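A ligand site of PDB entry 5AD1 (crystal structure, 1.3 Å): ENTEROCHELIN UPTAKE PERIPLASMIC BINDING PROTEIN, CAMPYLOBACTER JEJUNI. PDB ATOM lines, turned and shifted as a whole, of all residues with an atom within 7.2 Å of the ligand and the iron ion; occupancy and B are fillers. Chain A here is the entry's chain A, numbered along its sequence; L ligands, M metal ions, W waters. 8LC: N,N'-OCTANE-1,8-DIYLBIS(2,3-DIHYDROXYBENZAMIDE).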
ATOM      1  N   ASN A  60       8.724  27.092 -24.305  1.00  0.00           N
ATOM      2  CA  ASN A  60       8.144  25.826 -24.690  1.00  0.00           C
ATOM      3  C   ASN A  60       9.211  24.846 -25.151  1.00  0.00           C
ATOM      4  O   ASN A  60       8.940  24.045 -26.016  1.00  0.00           O
ATOM      5  CB  ASN A  60       7.065  25.992 -25.751  1.00  0.00           C
ATOM      6  CG  ASN A  60       5.963  26.902 -25.328  1.00  0.00           C
ATOM      7  OD1 ASN A  60       5.822  28.014 -25.831  1.00  0.00           O
ATOM      8  ND2 ASN A  60       5.165  26.471 -24.442  1.00  0.00           N
ATOM      9  N   GLY A  76       7.871  32.112 -26.449  1.00  0.00           N
ATOM     10  CA  GLY A  76       7.131  30.883 -26.592  1.00  0.00           C
ATOM     11  C   GLY A  76       6.490  30.776 -27.956  1.00  0.00           C
ATOM     12  O   GLY A  76       6.428  31.762 -28.709  1.00  0.00           O
ATOM     13  N   VAL A  77       6.022  29.576 -28.294  1.00  0.00           N
ATOM     14  CA  VAL A  77       5.378  29.369 -29.591  1.00  0.00           C
ATOM     15  C   VAL A  77       4.130  30.224 -29.838  1.00  0.00           C
ATOM     16  O   VAL A  77       3.817  30.545 -30.976  1.00  0.00           O
ATOM     17  CB  VAL A  77       5.127  27.883 -29.917  1.00  0.00           C
ATOM     18  CG1 VAL A  77       6.496  27.168 -30.038  1.00  0.00           C
ATOM     19  CG2 VAL A  77       4.182  27.198 -28.934  1.00  0.00           C
ATOM     20  N   GLN A  78       3.470  30.554 -28.717  1.00  0.00           N
ATOM     21  CA  GLN A  78       2.307  31.479 -28.705  1.00  0.00           C
ATOM     22  C   GLN A  78       2.585  32.861 -28.119  1.00  0.00           C
ATOM     23  O   GLN A  78       1.653  33.659 -27.885  1.00  0.00           O
ATOM     24  CB  GLN A  78       1.237  30.899 -27.830  1.00  0.00           C
ATOM     25  CG  GLN A  78       0.722  29.703 -28.417  1.00  0.00           C
ATOM     26  CD  GLN A  78      -0.271  29.873 -29.541  1.00  0.00           C
ATOM     27  OE1 GLN A  78      -0.630  30.970 -29.870  1.00  0.00           O
ATOM     28  NE2 GLN A  78      -0.701  28.805 -30.119  1.00  0.00           N
ATOM     29  N   GLN A  79       3.823  33.108 -27.766  1.00  0.00           N
ATOM     30  CA  GLN A  79       4.238  34.351 -27.153  1.00  0.00           C
ATOM     31  C   GLN A  79       5.559  34.747 -27.759  1.00  0.00           C
ATOM     32  O   GLN A  79       6.613  34.714 -27.109  1.00  0.00           O
ATOM     33  CB  GLN A  79       4.450  34.241 -25.616  1.00  0.00           C
ATOM     34  CG  GLN A  79       3.232  33.944 -24.778  1.00  0.00           C
ATOM     35  CD  GLN A  79       3.615  33.689 -23.303  1.00  0.00           C
ATOM     36  OE1 GLN A  79       3.346  32.631 -22.747  1.00  0.00           O
ATOM     37  NE2 GLN A  79       4.323  34.623 -22.710  1.00  0.00           N
ATOM     38  N   SER A  96       5.917  27.618 -38.063  1.00  0.00           N
ATOM     39  CA  SER A  96       4.822  26.771 -38.500  1.00  0.00           C
ATOM     40  C   SER A  96       3.521  27.410 -38.260  1.00  0.00           C
ATOM     41  O   SER A  96       3.423  28.662 -38.171  1.00  0.00           O
ATOM     42  CB  SER A  96       4.995  25.376 -38.093  1.00  0.00           C
ATOM     43  OG  SER A  96       5.047  25.308 -36.708  1.00  0.00           O
ATOM     44  N   GLY A  97       2.486  26.577 -38.208  1.00  0.00           N
ATOM     45  CA  GLY A  97       1.164  27.131 -38.214  1.00  0.00           C
ATOM     46  C   GLY A  97       0.832  28.122 -37.115  1.00  0.00           C
ATOM     47  O   GLY A  97      -0.015  29.008 -37.314  1.00  0.00           O
ATOM     48  N   ARG A  98       1.424  27.957 -35.937  1.00  0.00           N
ATOM     49  CA  ARG A  98       1.125  28.900 -34.864  1.00  0.00           C
ATOM     50  C   ARG A  98       1.551  30.335 -35.148  1.00  0.00           C
ATOM     51  O   ARG A  98       1.024  31.287 -34.532  1.00  0.00           O
ATOM     52  CB  ARG A  98       1.769  28.456 -33.527  1.00  0.00           C
ATOM     53  CG  ARG A  98       1.123  27.246 -32.905  1.00  0.00           C
ATOM     54  CD  ARG A  98       1.918  26.855 -31.686  1.00  0.00           C
ATOM     55  NE  ARG A  98       1.332  25.743 -30.947  1.00  0.00           N
ATOM     56  CZ  ARG A  98       1.678  24.459 -31.094  1.00  0.00           C
ATOM     57  NH1 ARG A  98       2.647  24.089 -31.955  1.00  0.00           N
ATOM     58  NH2 ARG A  98       0.994  23.597 -30.390  1.00  0.00           N
ATOM     59  N   GLN A  99       2.568  30.509 -36.015  1.00  0.00           N
ATOM     60  CA  GLN A  99       3.079  31.829 -36.267  1.00  0.00           C
ATOM     61  C   GLN A  99       2.702  32.376 -37.659  1.00  0.00           C
ATOM     62  O   GLN A  99       3.103  33.529 -37.946  1.00  0.00           O
ATOM     63  CB  GLN A  99       4.583  31.911 -36.069  1.00  0.00           C
ATOM     64  CG  GLN A  99       5.080  31.417 -34.714  1.00  0.00           C
ATOM     65  CD  GLN A  99       5.329  29.938 -34.635  1.00  0.00           C
ATOM     66  OE1 GLN A  99       5.673  29.255 -35.645  1.00  0.00           O
ATOM     67  NE2 GLN A  99       5.199  29.400 -33.433  1.00  0.00           N
ATOM     68  N   SER A 100       1.958  31.622 -38.477  1.00  0.00           N
ATOM     69  CA  SER A 100       1.480  32.187 -39.762  1.00  0.00           C
ATOM     70  C   SER A 100       0.830  33.543 -39.669  1.00  0.00           C
ATOM     71  O   SER A 100       0.997  34.400 -40.515  1.00  0.00           O
ATOM     72  CB  SER A 100       0.477  31.203 -40.404  1.00  0.00           C
ATOM     73  OG  SER A 100       1.129  30.067 -40.675  1.00  0.00           O
ATOM     74  N   LYS A 101       0.128  33.763 -38.558  1.00  0.00           N
ATOM     75  CA  LYS A 101      -0.601  34.998 -38.374  1.00  0.00           C
ATOM     76  C   LYS A 101       0.341  36.206 -38.198  1.00  0.00           C
ATOM     77  O   LYS A 101      -0.150  37.339 -38.296  1.00  0.00           O
ATOM     78  CB  LYS A 101      -1.565  34.896 -37.184  1.00  0.00           C
ATOM     79  CG  LYS A 101      -0.901  34.795 -35.811  1.00  0.00           C
ATOM     80  CD  LYS A 101      -1.891  34.594 -34.644  1.00  0.00           C
ATOM     81  CE  LYS A 101      -2.583  33.253 -34.637  1.00  0.00           C
ATOM     82  NZ  LYS A 101      -1.690  32.100 -34.336  1.00  0.00           N
ATOM     83  N   ASN A 173      -8.064  19.819 -21.693  1.00  0.00           N
ATOM     84  CA  ASN A 173      -7.701  21.153 -21.331  1.00  0.00           C
ATOM     85  C   ASN A 173      -8.669  21.660 -20.293  1.00  0.00           C
ATOM     86  O   ASN A 173      -9.880  21.567 -20.509  1.00  0.00           O
ATOM     87  CB  ASN A 173      -7.585  22.130 -22.509  1.00  0.00           C
ATOM     88  CG  ASN A 173      -6.836  23.451 -22.075  1.00  0.00           C
ATOM     89  OD1 ASN A 173      -5.649  23.438 -21.543  1.00  0.00           O
ATOM     90  ND2 ASN A 173      -7.592  24.520 -22.047  1.00  0.00           N
ATOM     91  N   ARG A 185      -4.517  16.930 -36.560  1.00  0.00           N
ATOM     92  CA  ARG A 185      -3.158  17.210 -36.098  1.00  0.00           C
ATOM     93  C   ARG A 185      -2.471  16.026 -35.414  1.00  0.00           C
ATOM     94  O   ARG A 185      -1.257  16.049 -35.226  1.00  0.00           O
ATOM     95  CB  ARG A 185      -3.152  18.397 -35.185  1.00  0.00           C
ATOM     96  CG  ARG A 185      -3.856  18.167 -33.854  1.00  0.00           C
ATOM     97  CD  ARG A 185      -3.975  19.442 -33.020  1.00  0.00           C
ATOM     98  NE  ARG A 185      -2.659  19.982 -32.638  1.00  0.00           N
ATOM     99  CZ  ARG A 185      -2.479  21.217 -32.141  1.00  0.00           C
ATOM    100  NH1 ARG A 185      -3.470  22.062 -32.011  1.00  0.00           N
ATOM    101  NH2 ARG A 185      -1.245  21.644 -31.849  1.00  0.00           N
ATOM    102  N   THR A 206      -8.797  23.376 -34.569  1.00  0.00           N
ATOM    103  CA  THR A 206      -7.411  23.367 -34.143  1.00  0.00           C
ATOM    104  C   THR A 206      -7.274  22.665 -32.780  1.00  0.00           C
ATOM    105  O   THR A 206      -6.313  21.865 -32.591  1.00  0.00           O
ATOM    106  CB  THR A 206      -6.846  24.779 -34.059  1.00  0.00           C
ATOM    107  OG1 THR A 206      -6.893  25.382 -35.385  1.00  0.00           O
ATOM    108  CG2 THR A 206      -5.445  24.847 -33.556  1.00  0.00           C
ATOM    109  N   HIS A 207      -8.199  22.945 -31.861  1.00  0.00           N
ATOM    110  CA  HIS A 207      -8.173  22.366 -30.525  1.00  0.00           C
ATOM    111  C   HIS A 207      -9.249  21.324 -30.288  1.00  0.00           C
ATOM    112  O   HIS A 207      -9.490  20.946 -29.129  1.00  0.00           O
ATOM    113  CB  HIS A 207      -8.085  23.440 -29.438  1.00  0.00           C
ATOM    114  CG  HIS A 207      -6.881  24.338 -29.605  1.00  0.00           C
ATOM    115  ND1 HIS A 207      -6.928  25.536 -30.262  1.00  0.00           N
ATOM    116  CD2 HIS A 207      -5.608  24.187 -29.195  1.00  0.00           C
ATOM    117  CE1 HIS A 207      -5.714  26.057 -30.261  1.00  0.00           C
ATOM    118  NE2 HIS A 207      -4.910  25.268 -29.621  1.00  0.00           N
ATOM    119  N   ARG A 229      -3.166  18.688 -22.872  1.00  0.00           N
ATOM    120  CA  ARG A 229      -2.759  20.095 -23.131  1.00  0.00           C
ATOM    121  C   ARG A 229      -2.560  20.895 -21.866  1.00  0.00           C
ATOM    122  O   ARG A 229      -1.819  21.897 -21.869  1.00  0.00           O
ATOM    123  CB  ARG A 229      -3.814  20.714 -24.069  1.00  0.00           C
ATOM    124  CG  ARG A 229      -3.545  22.156 -24.518  1.00  0.00           C
ATOM    125  CD  ARG A 229      -4.563  22.525 -25.574  1.00  0.00           C
ATOM    126  NE  ARG A 229      -4.402  23.889 -26.073  1.00  0.00           N
ATOM    127  CZ  ARG A 229      -5.171  24.929 -25.756  1.00  0.00           C
ATOM    128  NH1 ARG A 229      -6.175  24.789 -24.907  1.00  0.00           N
ATOM    129  NH2 ARG A 229      -4.961  26.120 -26.312  1.00  0.00           N
ATOM    130  N   ILE A 232       1.082  21.566 -21.183  1.00  0.00           N
ATOM    131  CA  ILE A 232       1.748  22.555 -22.060  1.00  0.00           C
ATOM    132  C   ILE A 232       1.380  23.979 -21.580  1.00  0.00           C
ATOM    133  O   ILE A 232       2.221  24.829 -21.496  1.00  0.00           O
ATOM    134  CB  ILE A 232       1.334  22.355 -23.505  1.00  0.00           C
ATOM    135  CG1 ILE A 232       1.660  20.935 -23.971  1.00  0.00           C
ATOM    136  CG2 ILE A 232       1.978  23.415 -24.409  1.00  0.00           C
ATOM    137  CD1 ILE A 232       3.091  20.476 -23.857  1.00  0.00           C
ATOM    138  N   LEU A 233       0.112  24.197 -21.178  1.00  0.00           N
ATOM    139  CA  LEU A 233      -0.381  25.500 -20.810  1.00  0.00           C
ATOM    140  C   LEU A 233      -0.122  25.853 -19.360  1.00  0.00           C
ATOM    141  O   LEU A 233      -0.232  27.008 -18.956  1.00  0.00           O
ATOM    142  CB  LEU A 233      -1.859  25.627 -21.161  1.00  0.00           C
ATOM    143  CG  LEU A 233      -2.170  26.133 -22.578  1.00  0.00           C
ATOM    144  CD1 LEU A 233      -1.578  25.205 -23.633  1.00  0.00           C
ATOM    145  CD2 LEU A 233      -3.712  26.266 -22.759  1.00  0.00           C
ATOM    146  N   TYR A 268       1.715  17.546 -29.123  1.00  0.00           N
ATOM    147  CA  TYR A 268       1.101  18.840 -29.285  1.00  0.00           C
ATOM    148  C   TYR A 268       2.048  19.961 -29.772  1.00  0.00           C
ATOM    149  O   TYR A 268       1.633  20.787 -30.550  1.00  0.00           O
ATOM    150  CB  TYR A 268       0.465  19.228 -27.937  1.00  0.00           C
ATOM    151  CG  TYR A 268      -0.388  20.478 -27.989  1.00  0.00           C
ATOM    152  CD1 TYR A 268      -1.653  20.417 -28.540  1.00  0.00           C
ATOM    153  CD2 TYR A 268       0.049  21.701 -27.504  1.00  0.00           C
ATOM    154  CE1 TYR A 268      -2.452  21.527 -28.602  1.00  0.00           C
ATOM    155  CE2 TYR A 268      -0.750  22.829 -27.594  1.00  0.00           C
ATOM    156  CZ  TYR A 268      -2.006  22.777 -28.147  1.00  0.00           C
ATOM    157  OH  TYR A 268      -2.748  23.896 -28.236  1.00  0.00           O
ATOM    158  N   LEU A 269       3.264  19.969 -29.238  1.00  0.00           N
ATOM    159  CA  LEU A 269       4.254  20.988 -29.613  1.00  0.00           C
ATOM    160  C   LEU A 269       5.033  20.672 -30.913  1.00  0.00           C
ATOM    161  O   LEU A 269       4.958  21.418 -31.868  1.00  0.00           O
ATOM    162  CB  LEU A 269       5.235  21.282 -28.484  1.00  0.00           C
ATOM    163  CG  LEU A 269       4.666  22.050 -27.300  1.00  0.00           C
ATOM    164  CD1 LEU A 269       5.805  22.139 -26.319  1.00  0.00           C
ATOM    165  CD2 LEU A 269       4.179  23.449 -27.668  1.00  0.00           C
ATOM    166  N   SER A 271       4.526  18.078 -32.866  1.00  0.00           N
ATOM    167  CA  SER A 271       3.527  17.620 -33.831  1.00  0.00           C
ATOM    168  C   SER A 271       4.029  16.571 -34.816  1.00  0.00           C
ATOM    169  O   SER A 271       3.490  16.461 -35.881  1.00  0.00           O
ATOM    170  CB  SER A 271       2.837  18.780 -34.497  1.00  0.00           C
ATOM    171  OG  SER A 271       2.305  19.663 -33.526  1.00  0.00           O
HETATM  172  C2  8LC L   1      -2.482  26.512 -32.217  1.00  0.00           C
HETATM  173  C3  8LC L   1      -2.439  27.357 -33.335  1.00  0.00           C
HETATM  174  C4  8LC L   1      -2.060  26.790 -34.575  1.00  0.00           C
HETATM  175  C5  8LC L   1      -1.651  25.488 -34.681  1.00  0.00           C
HETATM  176  C6  8LC L   1      -1.702  24.649 -33.573  1.00  0.00           C
HETATM  177  C7  8LC L   1      -2.090  25.151 -32.358  1.00  0.00           C
HETATM  178  C8  8LC L   1      -2.827  28.802 -33.302  1.00  0.00           C
HETATM  179  O9  8LC L   1      -2.755  29.554 -34.284  1.00  0.00           O
HETATM  180  N10 8LC L   1      -3.278  29.241 -32.120  1.00  0.00           N
HETATM  181  C11 8LC L   1      -3.698  30.610 -31.903  1.00  0.00           C
HETATM  182  C12 8LC L   1      -4.593  30.730 -30.662  1.00  0.00           C
HETATM  183  C13 8LC L   1      -4.831  32.136 -30.300  1.00  0.00           C
HETATM  184  C14 8LC L   1      -5.918  32.389 -29.247  1.00  0.00           C
HETATM  185  C15 8LC L   1      -5.786  31.526 -27.973  1.00  0.00           C
HETATM  186  C16 8LC L   1      -4.429  31.710 -27.333  1.00  0.00           C
HETATM  187  C17 8LC L   1      -4.366  31.193 -25.866  1.00  0.00           C
HETATM  188  C18 8LC L   1      -4.562  29.671 -25.809  1.00  0.00           C
HETATM  189  N19 8LC L   1      -3.435  28.941 -26.305  1.00  0.00           N
HETATM  190  C20 8LC L   1      -2.324  28.696 -25.576  1.00  0.00           C
HETATM  191  C21 8LC L   1      -1.298  27.808 -26.196  1.00  0.00           C
HETATM  192  C22 8LC L   1      -1.478  27.033 -27.369  1.00  0.00           C
HETATM  193  C23 8LC L   1      -0.438  26.337 -27.976  1.00  0.00           C
HETATM  194  C24 8LC L   1       0.831  26.325 -27.336  1.00  0.00           C
HETATM  195  C25 8LC L   1       0.997  27.045 -26.156  1.00  0.00           C
HETATM  196  C26 8LC L   1      -0.029  27.800 -25.602  1.00  0.00           C
HETATM  197  O27 8LC L   1      -2.139  29.214 -24.451  1.00  0.00           O
HETATM  198  O29 8LC L   1      -2.206  24.391 -31.240  1.00  0.00           O
HETATM  199  O30 8LC L   1      -2.693  26.965 -27.953  1.00  0.00           O
HETATM  200  O31 8LC L   1      -0.637  25.695 -29.140  1.00  0.00           O
HETATM  201  O1  8LC L   1      -2.842  26.916 -30.976  1.00  0.00           O
HETATM  202 FE    FE M   1      -2.664  25.478 -29.509  1.00  0.00          FE
HETATM  203  O   HOH W   1      -3.892  28.946 -36.698  1.00  0.00           O
HETATM  204  O   HOH W   2      -7.045  27.528 -24.709  1.00  0.00           O
HETATM  205  O   HOH W   3      -0.404  31.352 -24.332  1.00  0.00           O
HETATM  206  O   HOH W   4      -3.546  29.840 -22.296  1.00  0.00           O
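NZ of Lys 101 is in hydrogen-bond range of O9 of the ligand (2.8 Å). An oxygen (O29) of the ligand sits close to the guanidinium group of Arg 185 (2.8 Å). A nitrogen (N10) of the ligand sits close to the side-chain amide nitrogen of Gln 78 (3.3 Å). An oxygen (O30) of the ligand sits close to the guanidinium group (NH2) of Arg 229 (2.9 Å). The guanidinium group of Arg 98 sits close to an oxygen (O31) of the ligand (2.7 Å).
The side-chain amide nitrogen of Gln 99 sits at hydrogen-bond distance from the backbone carbonyl oxygen of Val 77. ND2 of Asn 173 sits close to NH1 of Arg 229, 3.2 Å away. N of Val 77 lies within hydrogen-bond range of OD1 of Asn 60, at 2.9 Å. The side-chain hydroxyl of Tyr 268 lies close to the guanidinium group of Arg 229, 2.7 Å away. The backbone carbonyl oxygen (O) of Tyr 268 sits at hydrogen-bond distance from the guanidinium group (NH2) of Arg 185 (3.3 Å). NH2 of Arg 98 is in hydrogen-bond range of O of Tyr 268. O of Tyr 268 lies within hydrogen-bond range of OG of Ser 271, 3.3 Å away. NE2 of His 207 lies close to NH2 of Arg 229 (3.4 Å).
Residues that only touch the ligand: Thr 206 (3.6 Å), Leu 233 (3.6 Å) and Val 77 (3.8 Å). Hydrophobic or aromatic side chains within 4 Å of the ligand: Val 77, His 207, Leu 233 and Tyr 268. Of the 21 residues printed, 10 come within 4 Å of the ligand.
Gln 78 touches the iron ion (NE2 to FE, 3.9 Å). NH2 of Arg 229 touches the iron ion (3.99 Å). Four residues have an atom within 4 Å of the iron ion: Gln 78, His 207, Arg 229 and Tyr 268.
The iron ion is bound by the side-chain hydroxyl of Tyr 268 (2.0 Å), an oxygen (O1) of the ligand (2.1 Å), an oxygen (O31) of the ligand (2.1 Å), an oxygen (O29) of the ligand (2.1 Å), an oxygen (O30) of the ligand (2.2 Å) and a ring nitrogen (NE2) of His 207 (2.3 Å).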
